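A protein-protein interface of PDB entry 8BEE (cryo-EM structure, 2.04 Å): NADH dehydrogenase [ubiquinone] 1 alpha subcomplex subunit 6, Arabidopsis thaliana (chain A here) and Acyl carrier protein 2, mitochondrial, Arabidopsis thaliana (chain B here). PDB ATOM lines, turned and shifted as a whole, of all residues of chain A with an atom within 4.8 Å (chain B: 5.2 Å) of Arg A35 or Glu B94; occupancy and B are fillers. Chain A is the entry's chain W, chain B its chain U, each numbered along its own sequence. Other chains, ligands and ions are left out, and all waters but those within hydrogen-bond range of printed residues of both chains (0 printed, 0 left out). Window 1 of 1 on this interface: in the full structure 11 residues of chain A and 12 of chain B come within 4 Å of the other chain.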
ATOM      1  N   ARG A  31     -23.165  -1.928 -30.605  1.00  0.00           N
ATOM      2  CA  ARG A  31     -24.158  -2.642 -29.808  1.00  0.00           C
ATOM      3  C   ARG A  31     -25.268  -1.707 -29.345  1.00  0.00           C
ATOM      4  O   ARG A  31     -26.454  -2.048 -29.431  1.00  0.00           O
ATOM      5  CB  ARG A  31     -23.488  -3.312 -28.611  1.00  0.00           C
ATOM      6  CG  ARG A  31     -22.743  -4.578 -28.970  1.00  0.00           C
ATOM      7  CD  ARG A  31     -22.268  -5.311 -27.739  1.00  0.00           C
ATOM      8  NE  ARG A  31     -20.951  -5.895 -27.948  1.00  0.00           N
ATOM      9  CZ  ARG A  31     -19.809  -5.289 -27.655  1.00  0.00           C
ATOM     10  NH1 ARG A  31     -19.786  -4.080 -27.120  1.00  0.00           N
ATOM     11  NH2 ARG A  31     -18.663  -5.912 -27.905  1.00  0.00           N
ATOM     12  N   ALA A  32     -24.904  -0.516 -28.860  1.00  0.00           N
ATOM     13  CA  ALA A  32     -25.920   0.429 -28.404  1.00  0.00           C
ATOM     14  C   ALA A  32     -26.825   0.867 -29.550  1.00  0.00           C
ATOM     15  O   ALA A  32     -28.037   1.022 -29.368  1.00  0.00           O
ATOM     16  CB  ALA A  32     -25.259   1.639 -27.745  1.00  0.00           C
ATOM     17  N   ALA A  33     -26.255   1.072 -30.739  1.00  0.00           N
ATOM     18  CA  ALA A  33     -27.058   1.476 -31.888  1.00  0.00           C
ATOM     19  C   ALA A  33     -28.011   0.366 -32.312  1.00  0.00           C
ATOM     20  O   ALA A  33     -29.183   0.621 -32.605  1.00  0.00           O
ATOM     21  CB  ALA A  33     -26.154   1.880 -33.052  1.00  0.00           C
ATOM     22  N   CYS A  34     -27.524  -0.875 -32.354  1.00  0.00           N
ATOM     23  CA  CYS A  34     -28.388  -1.976 -32.766  1.00  0.00           C
ATOM     24  C   CYS A  34     -29.501  -2.231 -31.759  1.00  0.00           C
ATOM     25  O   CYS A  34     -30.642  -2.499 -32.148  1.00  0.00           O
ATOM     26  CB  CYS A  34     -27.573  -3.245 -32.975  1.00  0.00           C
ATOM     27  SG  CYS A  34     -28.601  -4.593 -33.574  1.00  0.00           S
ATOM     28  N   ARG A  35     -29.194  -2.156 -30.463  1.00  0.00           N
ATOM     29  CA  ARG A  35     -30.209  -2.441 -29.455  1.00  0.00           C
ATOM     30  C   ARG A  35     -31.348  -1.430 -29.470  1.00  0.00           C
ATOM     31  O   ARG A  35     -32.431  -1.726 -28.958  1.00  0.00           O
ATOM     32  CB  ARG A  35     -29.569  -2.492 -28.068  1.00  0.00           C
ATOM     33  CG  ARG A  35     -28.714  -3.725 -27.859  1.00  0.00           C
ATOM     34  CD  ARG A  35     -28.121  -3.783 -26.471  1.00  0.00           C
ATOM     35  NE  ARG A  35     -27.518  -5.084 -26.219  1.00  0.00           N
ATOM     36  CZ  ARG A  35     -26.226  -5.279 -25.998  1.00  0.00           C
ATOM     37  NH1 ARG A  35     -25.372  -4.270 -25.964  1.00  0.00           N
ATOM     38  NH2 ARG A  35     -25.779  -6.518 -25.821  1.00  0.00           N
ATOM     39  N   SER A  36     -31.134  -0.253 -30.050  1.00  0.00           N
ATOM     40  CA  SER A  36     -32.163   0.772 -30.135  1.00  0.00           C
ATOM     41  C   SER A  36     -33.024   0.650 -31.388  1.00  0.00           C
ATOM     42  O   SER A  36     -33.873   1.515 -31.623  1.00  0.00           O
ATOM     43  CB  SER A  36     -31.519   2.160 -30.082  1.00  0.00           C
ATOM     44  OG  SER A  36     -31.303   2.666 -31.383  1.00  0.00           O
ATOM     45  N   ILE A  37     -32.814  -0.387 -32.200  1.00  0.00           N
ATOM     46  CA  ILE A  37     -33.583  -0.528 -33.439  1.00  0.00           C
ATOM     47  C   ILE A  37     -35.077  -0.716 -33.189  1.00  0.00           C
ATOM     48  O   ILE A  37     -35.879  -0.079 -33.890  1.00  0.00           O
ATOM     49  CB  ILE A  37     -32.977  -1.644 -34.311  1.00  0.00           C
ATOM     50  CG1 ILE A  37     -31.724  -1.133 -35.019  1.00  0.00           C
ATOM     51  CG2 ILE A  37     -33.977  -2.131 -35.343  1.00  0.00           C
ATOM     52  CD1 ILE A  37     -30.871  -2.229 -35.598  1.00  0.00           C
ATOM     53  N   PRO A  38     -35.523  -1.579 -32.261  1.00  0.00           N
ATOM     54  CA  PRO A  38     -36.980  -1.704 -32.045  1.00  0.00           C
ATOM     55  C   PRO A  38     -37.657  -0.405 -31.631  1.00  0.00           C
ATOM     56  O   PRO A  38     -38.779  -0.121 -32.077  1.00  0.00           O
ATOM     57  CB  PRO A  38     -37.074  -2.770 -30.945  1.00  0.00           C
ATOM     58  CG  PRO A  38     -35.837  -3.567 -31.094  1.00  0.00           C
ATOM     59  CD  PRO A  38     -34.777  -2.581 -31.477  1.00  0.00           C
ATOM     60  N   VAL B  90     -23.810 -12.223 -33.284  1.00  0.00           N
ATOM     61  CA  VAL B  90     -24.261 -12.349 -31.901  1.00  0.00           C
ATOM     62  C   VAL B  90     -25.433 -11.410 -31.632  1.00  0.00           C
ATOM     63  O   VAL B  90     -26.386 -11.773 -30.929  1.00  0.00           O
ATOM     64  CB  VAL B  90     -23.097 -12.103 -30.926  1.00  0.00           C
ATOM     65  CG1 VAL B  90     -23.612 -12.004 -29.503  1.00  0.00           C
ATOM     66  CG2 VAL B  90     -22.076 -13.216 -31.043  1.00  0.00           C
ATOM     67  N   MET B  91     -25.393 -10.198 -32.193  1.00  0.00           N
ATOM     68  CA  MET B  91     -26.525  -9.291 -32.032  1.00  0.00           C
ATOM     69  C   MET B  91     -27.763  -9.844 -32.726  1.00  0.00           C
ATOM     70  O   MET B  91     -28.890  -9.602 -32.281  1.00  0.00           O
ATOM     71  CB  MET B  91     -26.204  -7.902 -32.585  1.00  0.00           C
ATOM     72  CG  MET B  91     -25.274  -7.064 -31.709  1.00  0.00           C
ATOM     73  SD  MET B  91     -25.979  -6.450 -30.162  1.00  0.00           S
ATOM     74  CE  MET B  91     -27.610  -5.930 -30.655  1.00  0.00           C
ATOM     75  N   ALA B  92     -27.567 -10.562 -33.834  1.00  0.00           N
ATOM     76  CA  ALA B  92     -28.681 -11.240 -34.492  1.00  0.00           C
ATOM     77  C   ALA B  92     -29.263 -12.329 -33.602  1.00  0.00           C
ATOM     78  O   ALA B  92     -30.480 -12.539 -33.580  1.00  0.00           O
ATOM     79  CB  ALA B  92     -28.229 -11.824 -35.829  1.00  0.00           C
ATOM     80  N   LEU B  93     -28.404 -13.038 -32.863  1.00  0.00           N
ATOM     81  CA  LEU B  93     -28.887 -14.029 -31.905  1.00  0.00           C
ATOM     82  C   LEU B  93     -29.813 -13.398 -30.872  1.00  0.00           C
ATOM     83  O   LEU B  93     -30.740 -14.055 -30.387  1.00  0.00           O
ATOM     84  CB  LEU B  93     -27.710 -14.708 -31.199  1.00  0.00           C
ATOM     85  CG  LEU B  93     -26.912 -15.796 -31.926  1.00  0.00           C
ATOM     86  CD1 LEU B  93     -25.930 -16.459 -30.973  1.00  0.00           C
ATOM     87  CD2 LEU B  93     -27.824 -16.830 -32.552  1.00  0.00           C
ATOM     88  N   GLU B  94     -29.570 -12.133 -30.521  1.00  0.00           N
ATOM     89  CA  GLU B  94     -30.393 -11.451 -29.523  1.00  0.00           C
ATOM     90  C   GLU B  94     -31.805 -11.197 -30.033  1.00  0.00           C
ATOM     91  O   GLU B  94     -32.785 -11.407 -29.311  1.00  0.00           O
ATOM     92  CB  GLU B  94     -29.736 -10.133 -29.122  1.00  0.00           C
ATOM     93  CG  GLU B  94     -28.494 -10.302 -28.298  1.00  0.00           C
ATOM     94  CD  GLU B  94     -27.646  -9.049 -28.244  1.00  0.00           C
ATOM     95  OE1 GLU B  94     -26.533  -9.075 -28.805  1.00  0.00           O
ATOM     96  OE2 GLU B  94     -28.095  -8.041 -27.657  1.00  0.00           O
ATOM     97  N   GLU B  95     -31.928 -10.715 -31.272  1.00  0.00           N
ATOM     98  CA  GLU B  95     -33.250 -10.414 -31.808  1.00  0.00           C
ATOM     99  C   GLU B  95     -34.085 -11.677 -31.962  1.00  0.00           C
ATOM    100  O   GLU B  95     -35.270 -11.693 -31.614  1.00  0.00           O
ATOM    101  CB  GLU B  95     -33.123  -9.690 -33.147  1.00  0.00           C
ATOM    102  CG  GLU B  95     -34.420  -9.620 -33.938  1.00  0.00           C
ATOM    103  CD  GLU B  95     -34.189  -9.357 -35.412  1.00  0.00           C
ATOM    104  OE1 GLU B  95     -33.062  -8.962 -35.775  1.00  0.00           O
ATOM    105  OE2 GLU B  95     -35.134  -9.548 -36.205  1.00  0.00           O
ATOM    106  N   GLU B  96     -33.480 -12.751 -32.468  1.00  0.00           N
ATOM    107  CA  GLU B  96     -34.234 -13.966 -32.743  1.00  0.00           C
ATOM    108  C   GLU B  96     -34.744 -14.642 -31.480  1.00  0.00           C
ATOM    109  O   GLU B  96     -35.784 -15.307 -31.530  1.00  0.00           O
ATOM    110  CB  GLU B  96     -33.377 -14.931 -33.554  1.00  0.00           C
ATOM    111  CG  GLU B  96     -33.152 -14.454 -34.976  1.00  0.00           C
ATOM    112  CD  GLU B  96     -34.454 -14.232 -35.722  1.00  0.00           C
ATOM    113  OE1 GLU B  96     -35.264 -15.179 -35.799  1.00  0.00           O
ATOM    114  OE2 GLU B  96     -34.667 -13.112 -36.233  1.00  0.00           O
ATOM    115  N   PHE B  97     -34.046 -14.494 -30.358  1.00  0.00           N
ATOM    116  CA  PHE B  97     -34.487 -15.071 -29.098  1.00  0.00           C
ATOM    117  C   PHE B  97     -35.000 -14.023 -28.124  1.00  0.00           C
ATOM    118  O   PHE B  97     -35.312 -14.363 -26.979  1.00  0.00           O
ATOM    119  CB  PHE B  97     -33.355 -15.877 -28.453  1.00  0.00           C
ATOM    120  CG  PHE B  97     -33.077 -17.177 -29.148  1.00  0.00           C
ATOM    121  CD1 PHE B  97     -33.935 -18.253 -29.000  1.00  0.00           C
ATOM    122  CD2 PHE B  97     -31.970 -17.317 -29.966  1.00  0.00           C
ATOM    123  CE1 PHE B  97     -33.686 -19.448 -29.646  1.00  0.00           C
ATOM    124  CE2 PHE B  97     -31.715 -18.507 -30.612  1.00  0.00           C
ATOM    125  CZ  PHE B  97     -32.577 -19.577 -30.451  1.00  0.00           C
ATOM    126  N   GLY B  98     -35.071 -12.760 -28.538  1.00  0.00           N
ATOM    127  CA  GLY B  98     -35.822 -11.753 -27.820  1.00  0.00           C
ATOM    128  C   GLY B  98     -35.235 -11.270 -26.515  1.00  0.00           C
ATOM    129  O   GLY B  98     -35.968 -10.672 -25.718  1.00  0.00           O
ATOM    130  N   PHE B  99     -33.948 -11.489 -26.263  1.00  0.00           N
ATOM    131  CA  PHE B  99     -33.336 -11.022 -25.028  1.00  0.00           C
ATOM    132  C   PHE B  99     -31.884 -10.640 -25.274  1.00  0.00           C
ATOM    133  O   PHE B  99     -31.276 -11.032 -26.273  1.00  0.00           O
ATOM    134  CB  PHE B  99     -33.448 -12.072 -23.917  1.00  0.00           C
ATOM    135  CG  PHE B  99     -32.310 -13.042 -23.880  1.00  0.00           C
ATOM    136  CD1 PHE B  99     -32.203 -14.039 -24.829  1.00  0.00           C
ATOM    137  CD2 PHE B  99     -31.346 -12.962 -22.889  1.00  0.00           C
ATOM    138  CE1 PHE B  99     -31.153 -14.938 -24.795  1.00  0.00           C
ATOM    139  CE2 PHE B  99     -30.301 -13.855 -22.851  1.00  0.00           C
ATOM    140  CZ  PHE B  99     -30.205 -14.844 -23.805  1.00  0.00           C
ATOM    141  N   GLU B 100     -31.338  -9.859 -24.345  1.00  0.00           N
ATOM    142  CA  GLU B 100     -30.007  -9.276 -24.476  1.00  0.00           C
ATOM    143  C   GLU B 100     -28.966 -10.169 -23.812  1.00  0.00           C
ATOM    144  O   GLU B 100     -29.168 -10.644 -22.689  1.00  0.00           O
ATOM    145  CB  GLU B 100     -29.966  -7.872 -23.869  1.00  0.00           C
ATOM    146  CG  GLU B 100     -30.391  -7.790 -22.409  1.00  0.00           C
ATOM    147  CD  GLU B 100     -31.646  -6.963 -22.213  1.00  0.00           C
ATOM    148  OE1 GLU B 100     -32.542  -7.022 -23.081  1.00  0.00           O
ATOM    149  OE2 GLU B 100     -31.737  -6.251 -21.190  1.00  0.00           O
ATOM    150  N   ILE B 101     -27.860 -10.400 -24.512  1.00  0.00           N
ATOM    151  CA  ILE B 101     -26.773 -11.213 -23.977  1.00  0.00           C
ATOM    152  C   ILE B 101     -25.726 -10.275 -23.387  1.00  0.00           C
ATOM    153  O   ILE B 101     -25.322  -9.306 -24.045  1.00  0.00           O
ATOM    154  CB  ILE B 101     -26.168 -12.132 -25.050  1.00  0.00           C
ATOM    155  CG1 ILE B 101     -24.837 -12.700 -24.576  1.00  0.00           C
ATOM    156  CG2 ILE B 101     -25.926 -11.371 -26.328  1.00  0.00           C
ATOM    157  CD1 ILE B 101     -24.243 -13.697 -25.534  1.00  0.00           C
ATOM    158  N   ASP B 103     -22.478  -8.256 -22.330  1.00  0.00           N
ATOM    159  CA  ASP B 103     -21.256  -7.980 -23.079  1.00  0.00           C
ATOM    160  C   ASP B 103     -20.093  -8.818 -22.570  1.00  0.00           C
ATOM    161  O   ASP B 103     -19.280  -9.313 -23.359  1.00  0.00           O
ATOM    162  CB  ASP B 103     -20.922  -6.490 -23.000  1.00  0.00           C
ATOM    163  CG  ASP B 103     -20.259  -5.975 -24.259  1.00  0.00           C
ATOM    164  OD1 ASP B 103     -19.413  -6.700 -24.823  1.00  0.00           O
ATOM    165  OD2 ASP B 103     -20.584  -4.847 -24.684  1.00  0.00           O
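The side-chain carboxylate (OE2) of Glu B94 is in salt-bridge range of the guanidinium group (NH2) of Arg A35, 3.3 Å away. NH2 of Arg A35 sits at hydrogen-bond distance from O of Ile B101, at 3.3 Å. The guanidinium group (NH1) of Arg A31 lies within salt-bridge range of the side-chain carboxylate (OD2) of Asp B103 (2.7 Å).
The backbone NH of Phe B99 sits at hydrogen-bond distance from the backbone carbonyl oxygen of Glu B94 (3.3 Å).
Among the printed residues, merely in contact across the chains: Cys A34 with Met B91, Arg A35 with Met B91 and Arg A31 with Met B91.
Arg A35 touches just these residues of chain B: Met B91 (3.7 Å), Glu B94 (3.3 Å) and Ile B101 (3.3 Å). Glu B94 touches just one residue of chain A: Arg A35. Printed residues of chain A within 4 Å of Met B91: Arg A31, Cys A34 and Arg A35. Of the printed residues of chain A, Ile B101 touches Arg A35. Printed residues of chain A within 4 Å of Asp B103: Arg A31 (2.7 Å). Of the printed residues of chain B, Cys A34 touches Met B91 (3.4 Å). Printed residues of chain B within 4 Å of Arg A31: Met B91 and Asp B103. Val B90 touches none of the printed residues of chain A. The nearest printed residue of chain A that does not touch Ile B101 is Arg A31 (6.2 Å).
Of the 8 printed residues of chain A, 3 touch a printed residue of chain B. Along chain A the printed residues that touch a printed residue of chain B span positions 31 to 35. Printed residues of chain B that touch a printed residue of chain A: Met B91, Glu B94, Ile B101 and Asp B103. Among the printed residues, Asp or Glu carboxylates within 4 Å of a Lys or Arg side-chain nitrogen of the other chain: Arg A31 with Asp B103 (2.7 Å) and Arg A35 with Glu B94 (3.3 Å).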
